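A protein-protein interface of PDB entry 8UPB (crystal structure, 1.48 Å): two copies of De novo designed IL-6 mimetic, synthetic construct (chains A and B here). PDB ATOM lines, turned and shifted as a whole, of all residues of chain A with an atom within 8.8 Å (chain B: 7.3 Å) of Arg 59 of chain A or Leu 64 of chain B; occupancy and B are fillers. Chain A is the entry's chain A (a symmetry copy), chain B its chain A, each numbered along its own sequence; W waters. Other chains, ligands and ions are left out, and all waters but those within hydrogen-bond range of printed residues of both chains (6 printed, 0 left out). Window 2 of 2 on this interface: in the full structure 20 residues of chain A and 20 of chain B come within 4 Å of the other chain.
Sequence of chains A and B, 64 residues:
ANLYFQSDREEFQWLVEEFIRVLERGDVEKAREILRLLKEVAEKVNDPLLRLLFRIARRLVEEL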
ATOM      1  N   PHE A  19      31.534  -4.399  23.225  1.00  0.00           N
ATOM      2  CA  PHE A  19      31.134  -5.264  24.324  1.00  0.00           C
ATOM      3  C   PHE A  19      32.328  -5.642  25.184  1.00  0.00           C
ATOM      4  O   PHE A  19      32.278  -5.554  26.416  1.00  0.00           O
ATOM      5  CB  PHE A  19      30.504  -6.529  23.736  1.00  0.00           C
ATOM      6  CG  PHE A  19      30.187  -7.589  24.754  1.00  0.00           C
ATOM      7  CD1 PHE A  19      29.037  -7.515  25.521  1.00  0.00           C
ATOM      8  CD2 PHE A  19      31.031  -8.686  24.927  1.00  0.00           C
ATOM      9  CE1 PHE A  19      28.737  -8.506  26.453  1.00  0.00           C
ATOM     10  CE2 PHE A  19      30.732  -9.686  25.861  1.00  0.00           C
ATOM     11  CZ  PHE A  19      29.577  -9.591  26.620  1.00  0.00           C
ATOM     12  N   LEU A  23      32.889  -4.445  29.161  1.00  0.00           N
ATOM     13  CA  LEU A  23      32.927  -5.498  30.170  1.00  0.00           C
ATOM     14  C   LEU A  23      34.290  -5.562  30.849  1.00  0.00           C
ATOM     15  O   LEU A  23      34.373  -5.780  32.065  1.00  0.00           O
ATOM     16  CB  LEU A  23      32.530  -6.829  29.520  1.00  0.00           C
ATOM     17  CG  LEU A  23      32.709  -8.170  30.220  1.00  0.00           C
ATOM     18  CD1 LEU A  23      31.738  -9.163  29.608  1.00  0.00           C
ATOM     19  CD2 LEU A  23      34.158  -8.662  30.084  1.00  0.00           C
ATOM     20  N   ARG A  32      25.541  -5.667  29.167  1.00  0.00           N
ATOM     21  CA  ARG A  32      24.233  -6.288  28.974  1.00  0.00           C
ATOM     22  C   ARG A  32      23.440  -5.544  27.909  1.00  0.00           C
ATOM     23  O   ARG A  32      22.787  -6.162  27.058  1.00  0.00           O
ATOM     24  CB  ARG A  32      23.493  -6.331  30.319  1.00  0.00           C
ATOM     25  CG  ARG A  32      22.238  -7.203  30.338  1.00  0.00           C
ATOM     26  CD  ARG A  32      21.483  -7.172  31.690  1.00  0.00           C
ATOM     27  NE  ARG A  32      22.123  -7.959  32.744  1.00  0.00           N
ATOM     28  CZ  ARG A  32      21.922  -9.255  32.959  1.00  0.00           C
ATOM     29  NH1 ARG A  32      21.079  -9.962  32.222  1.00  0.00           N
ATOM     30  NH2 ARG A  32      22.599  -9.863  33.931  1.00  0.00           N
ATOM     31  N   LEU A  35      24.355  -6.519  24.392  1.00  0.00           N
ATOM     32  CA  LEU A  35      23.879  -7.830  23.945  1.00  0.00           C
ATOM     33  C   LEU A  35      22.733  -7.699  22.954  1.00  0.00           C
ATOM     34  O   LEU A  35      22.657  -8.444  21.969  1.00  0.00           O
ATOM     35  CB  LEU A  35      23.389  -8.664  25.136  1.00  0.00           C
ATOM     36  CG  LEU A  35      24.445  -9.157  26.118  1.00  0.00           C
ATOM     37  CD1 LEU A  35      23.748  -9.871  27.257  1.00  0.00           C
ATOM     38  CD2 LEU A  35      25.419 -10.093  25.405  1.00  0.00           C
ATOM     39  N   LEU A  52      26.190 -18.148  18.114  1.00  0.00           N
ATOM     40  CA  LEU A  52      26.938 -18.797  19.183  1.00  0.00           C
ATOM     41  C   LEU A  52      27.760 -17.790  19.979  1.00  0.00           C
ATOM     42  O   LEU A  52      27.908 -17.938  21.198  1.00  0.00           O
ATOM     43  CB  LEU A  52      27.835 -19.886  18.584  1.00  0.00           C
ATOM     44  CG  LEU A  52      27.061 -21.007  17.878  1.00  0.00           C
ATOM     45  CD1 LEU A  52      28.041 -21.916  17.152  1.00  0.00           C
ATOM     46  CD2 LEU A  52      26.242 -21.789  18.868  1.00  0.00           C
ATOM     47  N   LEU A  53      28.337 -16.780  19.307  1.00  0.00           N
ATOM     48  CA  LEU A  53      29.069 -15.749  20.041  1.00  0.00           C
ATOM     49  C   LEU A  53      28.138 -15.013  20.996  1.00  0.00           C
ATOM     50  O   LEU A  53      28.496 -14.772  22.156  1.00  0.00           O
ATOM     51  CB  LEU A  53      29.736 -14.758  19.077  1.00  0.00           C
ATOM     52  CG  LEU A  53      30.763 -13.804  19.721  1.00  0.00           C
ATOM     53  CD1 LEU A  53      31.762 -13.376  18.663  1.00  0.00           C
ATOM     54  CD2 LEU A  53      30.070 -12.594  20.355  1.00  0.00           C
ATOM     55  N   PHE A  54      26.942 -14.656  20.531  1.00  0.00           N
ATOM     56  CA  PHE A  54      25.942 -14.066  21.414  1.00  0.00           C
ATOM     57  C   PHE A  54      25.689 -14.955  22.627  1.00  0.00           C
ATOM     58  O   PHE A  54      25.645 -14.475  23.767  1.00  0.00           O
ATOM     59  CB  PHE A  54      24.640 -13.833  20.645  1.00  0.00           C
ATOM     60  CG  PHE A  54      23.481 -13.464  21.540  1.00  0.00           C
ATOM     61  CD1 PHE A  54      23.215 -12.131  21.840  1.00  0.00           C
ATOM     62  CD2 PHE A  54      22.687 -14.445  22.106  1.00  0.00           C
ATOM     63  CE1 PHE A  54      22.159 -11.782  22.688  1.00  0.00           C
ATOM     64  CE2 PHE A  54      21.635 -14.101  22.946  1.00  0.00           C
ATOM     65  CZ  PHE A  54      21.369 -12.781  23.231  1.00  0.00           C
ATOM     66  N   ARG A  55      25.539 -16.261  22.404  1.00  0.00           N
ATOM     67  CA  ARG A  55      25.231 -17.154  23.520  1.00  0.00           C
ATOM     68  C   ARG A  55      26.313 -17.115  24.587  1.00  0.00           C
ATOM     69  O   ARG A  55      26.012 -17.090  25.793  1.00  0.00           O
ATOM     70  CB  ARG A  55      25.107 -18.576  23.013  1.00  0.00           C
ATOM     71  CG  ARG A  55      24.651 -19.581  24.060  1.00  0.00           C
ATOM     72  CD  ARG A  55      24.143 -20.711  23.282  1.00  0.00           C
ATOM     73  NE  ARG A  55      23.849 -21.947  23.989  1.00  0.00           N
ATOM     74  CZ  ARG A  55      23.350 -22.993  23.350  1.00  0.00           C
ATOM     75  NH1 ARG A  55      23.046 -22.922  22.066  1.00  0.00           N
ATOM     76  NH2 ARG A  55      23.166 -24.136  24.005  1.00  0.00           N
ATOM     77  N   ILE A  56      27.578 -17.152  24.162  1.00  0.00           N
ATOM     78  CA  ILE A  56      28.708 -17.091  25.088  1.00  0.00           C
ATOM     79  C   ILE A  56      28.750 -15.731  25.771  1.00  0.00           C
ATOM     80  O   ILE A  56      28.920 -15.639  26.991  1.00  0.00           O
ATOM     81  CB  ILE A  56      30.015 -17.402  24.328  1.00  0.00           C
ATOM     82  CG1 ILE A  56      29.986 -18.834  23.783  1.00  0.00           C
ATOM     83  CG2 ILE A  56      31.242 -17.129  25.212  1.00  0.00           C
ATOM     84  CD1 ILE A  56      31.111 -19.134  22.793  1.00  0.00           C
ATOM     85  N   ALA A  57      28.565 -14.664  24.998  1.00  0.00           N
ATOM     86  CA  ALA A  57      28.603 -13.316  25.555  1.00  0.00           C
ATOM     87  C   ALA A  57      27.507 -13.127  26.595  1.00  0.00           C
ATOM     88  O   ALA A  57      27.734 -12.516  27.655  1.00  0.00           O
ATOM     89  CB  ALA A  57      28.427 -12.294  24.430  1.00  0.00           C
ATOM     90  N   ARG A  58      26.316 -13.653  26.309  1.00  0.00           N
ATOM     91  CA  ARG A  58      25.198 -13.485  27.228  1.00  0.00           C
ATOM     92  C   ARG A  58      25.458 -14.226  28.531  1.00  0.00           C
ATOM     93  O   ARG A  58      25.180 -13.703  29.617  1.00  0.00           O
ATOM     94  CB  ARG A  58      23.914 -13.963  26.577  1.00  0.00           C
ATOM     95  CG  ARG A  58      22.769 -13.767  27.521  1.00  0.00           C
ATOM     96  CD  ARG A  58      21.464 -14.091  26.876  1.00  0.00           C
ATOM     97  NE  ARG A  58      20.403 -14.075  27.872  1.00  0.00           N
ATOM     98  CZ  ARG A  58      19.986 -15.142  28.534  1.00  0.00           C
ATOM     99  NH1 ARG A  58      20.499 -16.343  28.303  1.00  0.00           N
ATOM    100  NH2 ARG A  58      19.032 -15.005  29.451  1.00  0.00           N
ATOM    101  N   ARG A  59      26.046 -15.419  28.443  1.00  0.00           N
ATOM    102  CA  ARG A  59      26.396 -16.183  29.638  1.00  0.00           C
ATOM    103  C   ARG A  59      27.480 -15.477  30.439  1.00  0.00           C
ATOM    104  O   ARG A  59      27.454 -15.481  31.678  1.00  0.00           O
ATOM    105  CB  ARG A  59      26.887 -17.573  29.220  1.00  0.00           C
ATOM    106  CG  ARG A  59      27.294 -18.493  30.380  1.00  0.00           C
ATOM    107  CD  ARG A  59      26.134 -18.686  31.345  1.00  0.00           C
ATOM    108  NE  ARG A  59      26.473 -19.579  32.447  1.00  0.00           N
ATOM    109  CZ  ARG A  59      26.314 -20.896  32.431  1.00  0.00           C
ATOM    110  NH1 ARG A  59      25.836 -21.525  31.365  1.00  0.00           N
ATOM    111  NH2 ARG A  59      26.640 -21.599  33.514  1.00  0.00           N
ATOM    112  N   LEU A  60      28.444 -14.869  29.754  1.00  0.00           N
ATOM    113  CA  LEU A  60      29.489 -14.132  30.451  1.00  0.00           C
ATOM    114  C   LEU A  60      28.888 -13.003  31.276  1.00  0.00           C
ATOM    115  O   LEU A  60      29.252 -12.817  32.440  1.00  0.00           O
ATOM    116  CB  LEU A  60      30.532 -13.599  29.467  1.00  0.00           C
ATOM    117  CG  LEU A  60      31.628 -12.694  30.051  1.00  0.00           C
ATOM    118  CD1 LEU A  60      32.351 -13.344  31.228  1.00  0.00           C
ATOM    119  CD2 LEU A  60      32.622 -12.294  28.940  1.00  0.00           C
ATOM    120  N   VAL A  61      27.950 -12.251  30.698  1.00  0.00           N
ATOM    121  CA  VAL A  61      27.308 -11.176  31.444  1.00  0.00           C
ATOM    122  C   VAL A  61      26.660 -11.718  32.710  1.00  0.00           C
ATOM    123  O   VAL A  61      26.767 -11.105  33.784  1.00  0.00           O
ATOM    124  CB  VAL A  61      26.314 -10.421  30.546  1.00  0.00           C
ATOM    125  CG1 VAL A  61      25.391  -9.525  31.390  1.00  0.00           C
ATOM    126  CG2 VAL A  61      27.085  -9.600  29.520  1.00  0.00           C
ATOM    127  N   GLU A  62      26.003 -12.882  32.613  1.00  0.00           N
ATOM    128  CA  GLU A  62      25.366 -13.493  33.780  1.00  0.00           C
ATOM    129  C   GLU A  62      26.381 -13.876  34.850  1.00  0.00           C
ATOM    130  O   GLU A  62      26.083 -13.793  36.049  1.00  0.00           O
ATOM    131  CB  GLU A  62      24.546 -14.721  33.370  1.00  0.00           C
ATOM    132  CG  GLU A  62      23.335 -14.426  32.500  1.00  0.00           C
ATOM    133  CD  GLU A  62      22.333 -13.480  33.158  1.00  0.00           C
ATOM    134  OE1 GLU A  62      22.372 -13.304  34.398  1.00  0.00           O
ATOM    135  OE2 GLU A  62      21.508 -12.902  32.420  1.00  0.00           O
ATOM    136  N   GLU A  63      27.587 -14.269  34.452  1.00  0.00           N
ATOM    137  CA  GLU A  63      28.563 -14.755  35.417  1.00  0.00           C
ATOM    138  C   GLU A  63      29.438 -13.659  36.011  1.00  0.00           C
ATOM    139  O   GLU A  63      30.173 -13.933  36.968  1.00  0.00           O
ATOM    140  CB  GLU A  63      29.451 -15.829  34.774  1.00  0.00           C
ATOM    141  CG  GLU A  63      28.709 -17.051  34.249  1.00  0.00           C
ATOM    142  CD  GLU A  63      27.966 -17.821  35.332  1.00  0.00           C
ATOM    143  OE1 GLU A  63      28.254 -17.618  36.531  1.00  0.00           O
ATOM    144  OE2 GLU A  63      27.088 -18.631  34.971  1.00  0.00           O
ATOM    145  N   LEU A  64      29.405 -12.443  35.468  1.00  0.00           N
ATOM    146  CA  LEU A  64      30.204 -11.347  36.008  1.00  0.00           C
ATOM    147  C   LEU A  64      29.540 -10.829  37.282  1.00  0.00           C
ATOM    148  O   LEU A  64      30.188 -10.668  38.316  1.00  0.00           O
ATOM    149  CB  LEU A  64      30.340 -10.211  34.991  1.00  0.00           C
ATOM    150  CG  LEU A  64      31.204 -10.421  33.747  1.00  0.00           C
ATOM    151  CD1 LEU A  64      30.977  -9.300  32.749  1.00  0.00           C
ATOM    152  CD2 LEU A  64      32.669 -10.502  34.139  1.00  0.00           C
ATOM    153  N   PHE B  19      32.516 -26.440  23.007  1.00  0.00           N
ATOM    154  CA  PHE B  19      32.807 -25.602  24.160  1.00  0.00           C
ATOM    155  C   PHE B  19      31.535 -25.243  24.909  1.00  0.00           C
ATOM    156  O   PHE B  19      31.466 -25.361  26.138  1.00  0.00           O
ATOM    157  CB  PHE B  19      33.489 -24.324  23.667  1.00  0.00           C
ATOM    158  CG  PHE B  19      33.705 -23.289  24.735  1.00  0.00           C
ATOM    159  CD1 PHE B  19      34.776 -23.383  25.608  1.00  0.00           C
ATOM    160  CD2 PHE B  19      32.848 -22.196  24.852  1.00  0.00           C
ATOM    161  CE1 PHE B  19      34.983 -22.415  26.588  1.00  0.00           C
ATOM    162  CE2 PHE B  19      33.053 -21.218  25.835  1.00  0.00           C
ATOM    163  CZ  PHE B  19      34.130 -21.333  26.700  1.00  0.00           C
ATOM    164  N   ILE B  20      30.522 -24.786  24.180  1.00  0.00           N
ATOM    165  CA  ILE B  20      29.251 -24.434  24.799  1.00  0.00           C
ATOM    166  C   ILE B  20      28.632 -25.651  25.472  1.00  0.00           C
ATOM    167  O   ILE B  20      28.165 -25.579  26.617  1.00  0.00           O
ATOM    168  CB  ILE B  20      28.326 -23.800  23.746  1.00  0.00           C
ATOM    169  CG1 ILE B  20      28.853 -22.415  23.336  1.00  0.00           C
ATOM    170  CG2 ILE B  20      26.888 -23.714  24.281  1.00  0.00           C
ATOM    171  CD1 ILE B  20      28.119 -21.805  22.157  1.00  0.00           C
ATOM    172  N   VAL B  22      30.002 -28.388  26.760  1.00  0.00           N
ATOM    173  CA  VAL B  22      30.646 -28.855  27.987  1.00  0.00           C
ATOM    174  C   VAL B  22      30.501 -27.831  29.108  1.00  0.00           C
ATOM    175  O   VAL B  22      30.309 -28.193  30.275  1.00  0.00           O
ATOM    176  CB  VAL B  22      32.111 -29.262  27.731  1.00  0.00           C
ATOM    177  CG1 VAL B  22      32.194 -30.335  26.645  1.00  0.00           C
ATOM    178  CG2 VAL B  22      32.966 -28.058  27.375  1.00  0.00           C
ATOM    179  N   LEU B  23      30.593 -26.535  28.783  1.00  0.00           N
ATOM    180  CA  LEU B  23      30.457 -25.507  29.809  1.00  0.00           C
ATOM    181  C   LEU B  23      29.034 -25.458  30.354  1.00  0.00           C
ATOM    182  O   LEU B  23      28.834 -25.269  31.561  1.00  0.00           O
ATOM    183  CB  LEU B  23      30.913 -24.161  29.233  1.00  0.00           C
ATOM    184  CG  LEU B  23      30.665 -22.837  29.944  1.00  0.00           C
ATOM    185  CD1 LEU B  23      31.690 -21.831  29.453  1.00  0.00           C
ATOM    186  CD2 LEU B  23      29.235 -22.340  29.681  1.00  0.00           C
ATOM    187  N   GLU B  24      28.031 -25.652  29.489  1.00  0.00           N
ATOM    188  CA  GLU B  24      26.644 -25.677  29.943  1.00  0.00           C
ATOM    189  C   GLU B  24      26.331 -26.925  30.762  1.00  0.00           C
ATOM    190  O   GLU B  24      25.386 -26.899  31.559  1.00  0.00           O
ATOM    191  CB  GLU B  24      25.699 -25.486  28.750  1.00  0.00           C
ATOM    192  CG  GLU B  24      25.755 -24.042  28.240  1.00  0.00           C
ATOM    193  CD  GLU B  24      24.849 -23.757  27.053  1.00  0.00           C
ATOM    194  OE1 GLU B  24      24.269 -24.703  26.483  1.00  0.00           O
ATOM    195  OE2 GLU B  24      24.724 -22.565  26.696  1.00  0.00           O
ATOM    196  N   ARG B  25      27.117 -27.995  30.616  1.00  0.00           N
ATOM    197  CA  ARG B  25      27.045 -29.147  31.508  1.00  0.00           C
ATOM    198  C   ARG B  25      27.760 -28.904  32.828  1.00  0.00           C
ATOM    199  O   ARG B  25      27.683 -29.755  33.723  1.00  0.00           O
ATOM    200  CB  ARG B  25      27.716 -30.366  30.872  1.00  0.00           C
ATOM    201  CG  ARG B  25      27.124 -30.804  29.564  1.00  0.00           C
ATOM    202  CD  ARG B  25      27.949 -31.930  28.965  1.00  0.00           C
ATOM    203  NE  ARG B  25      27.222 -33.193  28.980  1.00  0.00           N
ATOM    204  CZ  ARG B  25      27.355 -34.128  29.911  1.00  0.00           C
ATOM    205  NH1 ARG B  25      28.218 -33.995  30.906  1.00  0.00           N
ATOM    206  NH2 ARG B  25      26.604 -35.224  29.839  1.00  0.00           N
ATOM    207  N   GLY B  26      28.464 -27.787  32.955  1.00  0.00           N
ATOM    208  CA  GLY B  26      29.228 -27.494  34.147  1.00  0.00           C
ATOM    209  C   GLY B  26      30.616 -28.089  34.180  1.00  0.00           C
ATOM    210  O   GLY B  26      31.273 -28.025  35.229  1.00  0.00           O
ATOM    211  N   ASP B  27      31.100 -28.649  33.071  1.00  0.00           N
ATOM    212  CA  ASP B  27      32.447 -29.227  33.023  1.00  0.00           C
ATOM    213  C   ASP B  27      33.445 -28.135  32.643  1.00  0.00           C
ATOM    214  O   ASP B  27      33.909 -28.036  31.504  1.00  0.00           O
ATOM    215  CB  ASP B  27      32.508 -30.395  32.050  1.00  0.00           C
ATOM    216  CG  ASP B  27      33.866 -31.088  32.060  1.00  0.00           C
ATOM    217  OD1 ASP B  27      34.740 -30.708  32.883  1.00  0.00           O
ATOM    218  OD2 ASP B  27      34.060 -32.014  31.245  1.00  0.00           O
ATOM    219  N   VAL B  28      33.796 -27.321  33.641  1.00  0.00           N
ATOM    220  CA  VAL B  28      34.644 -26.154  33.407  1.00  0.00           C
ATOM    221  C   VAL B  28      36.053 -26.578  33.015  1.00  0.00           C
ATOM    222  O   VAL B  28      36.700 -25.934  32.180  1.00  0.00           O
ATOM    223  CB  VAL B  28      34.653 -25.246  34.651  1.00  0.00           C
ATOM    224  CG1 VAL B  28      35.612 -24.071  34.446  1.00  0.00           C
ATOM    225  CG2 VAL B  28      33.248 -24.755  34.975  1.00  0.00           C
ATOM    226  N   ALA B  31      35.962 -27.324  29.384  1.00  0.00           N
ATOM    227  CA  ALA B  31      35.804 -26.113  28.583  1.00  0.00           C
ATOM    228  C   ALA B  31      37.134 -25.389  28.440  1.00  0.00           C
ATOM    229  O   ALA B  31      37.472 -24.899  27.351  1.00  0.00           O
ATOM    230  CB  ALA B  31      34.764 -25.200  29.220  1.00  0.00           C
ATOM    231  N   ALA B  57      35.288 -16.224  25.305  1.00  0.00           N
ATOM    232  CA  ALA B  57      35.198 -17.585  25.823  1.00  0.00           C
ATOM    233  C   ALA B  57      36.188 -17.800  26.959  1.00  0.00           C
ATOM    234  O   ALA B  57      35.861 -18.436  27.977  1.00  0.00           O
ATOM    235  CB  ALA B  57      35.483 -18.580  24.696  1.00  0.00           C
ATOM    236  N   ARG B  59      37.460 -15.555  28.995  1.00  0.00           N
ATOM    237  CA  ARG B  59      36.996 -14.819  30.168  1.00  0.00           C
ATOM    238  C   ARG B  59      35.841 -15.543  30.844  1.00  0.00           C
ATOM    239  O   ARG B  59      35.746 -15.569  32.079  1.00  0.00           O
ATOM    240  CB  ARG B  59      36.546 -13.419  29.738  1.00  0.00           C
ATOM    241  CG  ARG B  59      36.027 -12.527  30.875  1.00  0.00           C
ATOM    242  CD  ARG B  59      37.089 -12.359  31.952  1.00  0.00           C
ATOM    243  NE  ARG B  59      36.644 -11.492  33.038  1.00  0.00           N
ATOM    244  CZ  ARG B  59      36.802 -10.176  33.069  1.00  0.00           C
ATOM    245  NH1 ARG B  59      37.380  -9.522  32.069  1.00  0.00           N
ATOM    246  NH2 ARG B  59      36.371  -9.498  34.131  1.00  0.00           N
ATOM    247  N   LEU B  60      34.948 -16.134  30.054  1.00  0.00           N
ATOM    248  CA  LEU B  60      33.841 -16.886  30.629  1.00  0.00           C
ATOM    249  C   LEU B  60      34.361 -18.035  31.481  1.00  0.00           C
ATOM    250  O   LEU B  60      33.886 -18.249  32.599  1.00  0.00           O
ATOM    251  CB  LEU B  60      32.898 -17.394  29.536  1.00  0.00           C
ATOM    252  CG  LEU B  60      31.752 -18.312  29.989  1.00  0.00           C
ATOM    253  CD1 LEU B  60      30.918 -17.689  31.106  1.00  0.00           C
ATOM    254  CD2 LEU B  60      30.871 -18.684  28.778  1.00  0.00           C
ATOM    255  N   VAL B  61      35.351 -18.774  30.978  1.00  0.00           N
ATOM    256  CA  VAL B  61      35.919 -19.868  31.757  1.00  0.00           C
ATOM    257  C   VAL B  61      36.441 -19.357  33.093  1.00  0.00           C
ATOM    258  O   VAL B  61      36.231 -19.995  34.136  1.00  0.00           O
ATOM    259  CB  VAL B  61      36.996 -20.601  30.941  1.00  0.00           C
ATOM    260  CG1 VAL B  61      37.835 -21.519  31.848  1.00  0.00           C
ATOM    261  CG2 VAL B  61      36.329 -21.397  29.826  1.00  0.00           C
ATOM    262  N   GLU B  62      37.103 -18.191  33.087  1.00  0.00           N
ATOM    263  CA  GLU B  62      37.624 -17.610  34.325  1.00  0.00           C
ATOM    264  C   GLU B  62      36.509 -17.251  35.301  1.00  0.00           C
ATOM    265  O   GLU B  62      36.690 -17.363  36.520  1.00  0.00           O
ATOM    266  CB  GLU B  62      38.478 -16.373  34.025  1.00  0.00           C
ATOM    267  CG  GLU B  62      39.767 -16.648  33.270  1.00  0.00           C
ATOM    268  CD  GLU B  62      40.702 -17.612  33.999  1.00  0.00           C
ATOM    269  OE1 GLU B  62      40.544 -17.817  35.225  1.00  0.00           O
ATOM    270  OE2 GLU B  62      41.596 -18.172  33.331  1.00  0.00           O
ATOM    271  N   GLU B  63      35.347 -16.847  34.797  1.00  0.00           N
ATOM    272  CA  GLU B  63      34.281 -16.384  35.674  1.00  0.00           C
ATOM    273  C   GLU B  63      33.354 -17.493  36.154  1.00  0.00           C
ATOM    274  O   GLU B  63      32.530 -17.241  37.042  1.00  0.00           O
ATOM    275  CB  GLU B  63      33.459 -15.294  34.974  1.00  0.00           C
ATOM    276  CG  GLU B  63      34.247 -14.060  34.554  1.00  0.00           C
ATOM    277  CD  GLU B  63      34.880 -13.317  35.721  1.00  0.00           C
ATOM    278  OE1 GLU B  63      34.478 -13.549  36.881  1.00  0.00           O
ATOM    279  OE2 GLU B  63      35.788 -12.500  35.467  1.00  0.00           O
ATOM    280  N   LEU B  64      33.441 -18.695  35.588  1.00  0.00           N
ATOM    281  CA  LEU B  64      32.595 -19.803  36.022  1.00  0.00           C
ATOM    282  C   LEU B  64      33.133 -20.352  37.341  1.00  0.00           C
ATOM    283  O   LEU B  64      32.388 -20.537  38.304  1.00  0.00           O
ATOM    284  CB  LEU B  64      32.560 -20.914  34.970  1.00  0.00           C
ATOM    285  CG  LEU B  64      31.819 -20.673  33.653  1.00  0.00           C
ATOM    286  CD1 LEU B  64      32.144 -21.770  32.655  1.00  0.00           C
ATOM    287  CD2 LEU B  64      30.323 -20.600  33.903  1.00  0.00           C
HETATM  288  O   HOH W   1      35.702  -6.646  34.096  1.00  0.00           O
HETATM  289  O   HOH W   2      24.369 -23.898  31.951  1.00  0.00           O
HETATM  290  O   HOH W   3      25.014 -20.607  28.463  1.00  0.00           O
HETATM  291  O   HOH W   4      32.503 -14.342  38.351  1.00  0.00           O
HETATM  292  O   HOH W   5      30.077 -16.862  38.203  1.00  0.00           O
HETATM  293  O   HOH W   6      27.313 -24.450  33.475  1.00  0.00           O
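The guanidinium group (NH2) of Arg 55 of chain A is in salt-bridge range of the side-chain carboxylate (OE1) of Glu 24 of chain B (2.8 Å).
The guanidinium group of Arg 59 of chain A lies within salt-bridge range of the side-chain carboxylate of Glu 63 of chain A (2.8 Å). The guanidinium group (NE) of Arg 59 of chain B is in salt-bridge range of the side-chain carboxylate (OE2) of Glu 63 of chain B, at 2.8 Å.
Leu 23 of chain A touches Arg 59 of chain B. Ile 56 of chain A touches Leu 60 of chain B (CG2 to CD2, 3.9 Å). CD2 of Leu 23 of chain B touches NH1 of Arg 59 of chain A (3.9 Å). CG of Arg 59 of chain A touches CD1 of Leu 60 of chain B (3.8 Å). Leu 64 of chain B touches Arg 59 of chain A. Leu 60 of chain A touches Arg 59 of chain B. CA of Leu 60 of chain A touches CD1 of Leu 60 of chain B, 3.9 Å away. Leu 60 of chain A touches Glu 63 of chain B (CD1 to CG, 3.9 Å). Leu 64 of chain B touches Glu 63 of chain A (CD2 to CG, 3.9 Å). Leu 64 of chain A touches Arg 59 of chain B (CD2 to NH2, 3.8 Å).
Of the printed residues of chain B, Arg 55 of chain A touches Ile 20 and Glu 24. Printed residues of chain B within 4 Å of Ile 56 of chain A: Ile 20 and Leu 60. Ala 57 of chain A touches none of the printed residues of chain B. Of the printed residues of chain B, Leu 60 of chain A touches Arg 59, Leu 60 and Glu 63. Printed residues of chain B within 4 Å of Leu 64 of chain A: Arg 59 (3.8 Å) and Glu 63 (3.9 Å). Of the printed residues of chain A, Leu 60 of chain B touches Ile 56, Arg 59, Leu 60 and Glu 63. Leu 64 of chain B touches just these residues of chain A: Arg 59 (3.8 Å) and Glu 63 (3.9 Å). The nearest residue of chain A that does not touch Leu 64 of chain B is Leu 60 of chain A (7.0 Å).
Of the 17 printed residues of chain B, 7 touch a printed residue of chain A. Of the 17 printed residues of chain A, 8 touch a printed residue of chain B. Printed residues of chain A that touch a printed residue of chain B: Leu 23, Leu 52, Arg 55, Ile 56, Arg 59, Leu 60, Glu 63 and Leu 64. Hydrophobic or aromatic side chains of chain A within 4 Å of the printed part of chain B: Leu 23, Leu 52, Ile 56, Leu 60 and Leu 64. Among the printed residues, 16 pairs touch across the chains.
Leu 23 of chain A touches Arg 59 of chain B, and with the chains exchanged Arg 59 of chain A touches Leu 23 of chain B. Arg 59 of chain A touches Leu 60 of chain B, and with the chains exchanged Leu 60 of chain A touches Arg 59 of chain B. Leu 60 of chain A touches its own counterpart, Leu 60 of chain B. Leu 60 of chain A touches Glu 63 of chain B, and with the chains exchanged Glu 63 of chain A touches Leu 60 of chain B.
Water W6 bridges the backbone carbonyl oxygen (O) of Leu 23 of chain B and the guanidinium group (NH2) of Arg 59 of chain A. Water W1 lies within hydrogen-bond range of the backbone carbonyl oxygen of Leu 23 of chain A (2.6 Å) and the guanidinium group of Arg 59 of chain B (2.9 Å). Water W4 lies within hydrogen-bond range of the side-chain carboxylate of Glu 63 of chain B and the backbone carbonyl oxygen of Glu 63 of chain A. Water W5 bridges the side-chain carboxylate of Glu 63 of chain A (2.6 Å) and the backbone carbonyl oxygen of Glu 63 of chain B (2.7 Å). Water W3 lies within hydrogen-bond range of OE2 of Glu 24 of chain B and NH1 of Arg 59 of chain A. Water W2 bridges the guanidinium group of Arg 59 of chain A (2.9 Å) and the backbone carbonyl oxygen of Glu 24 of chain B (3.2 Å).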
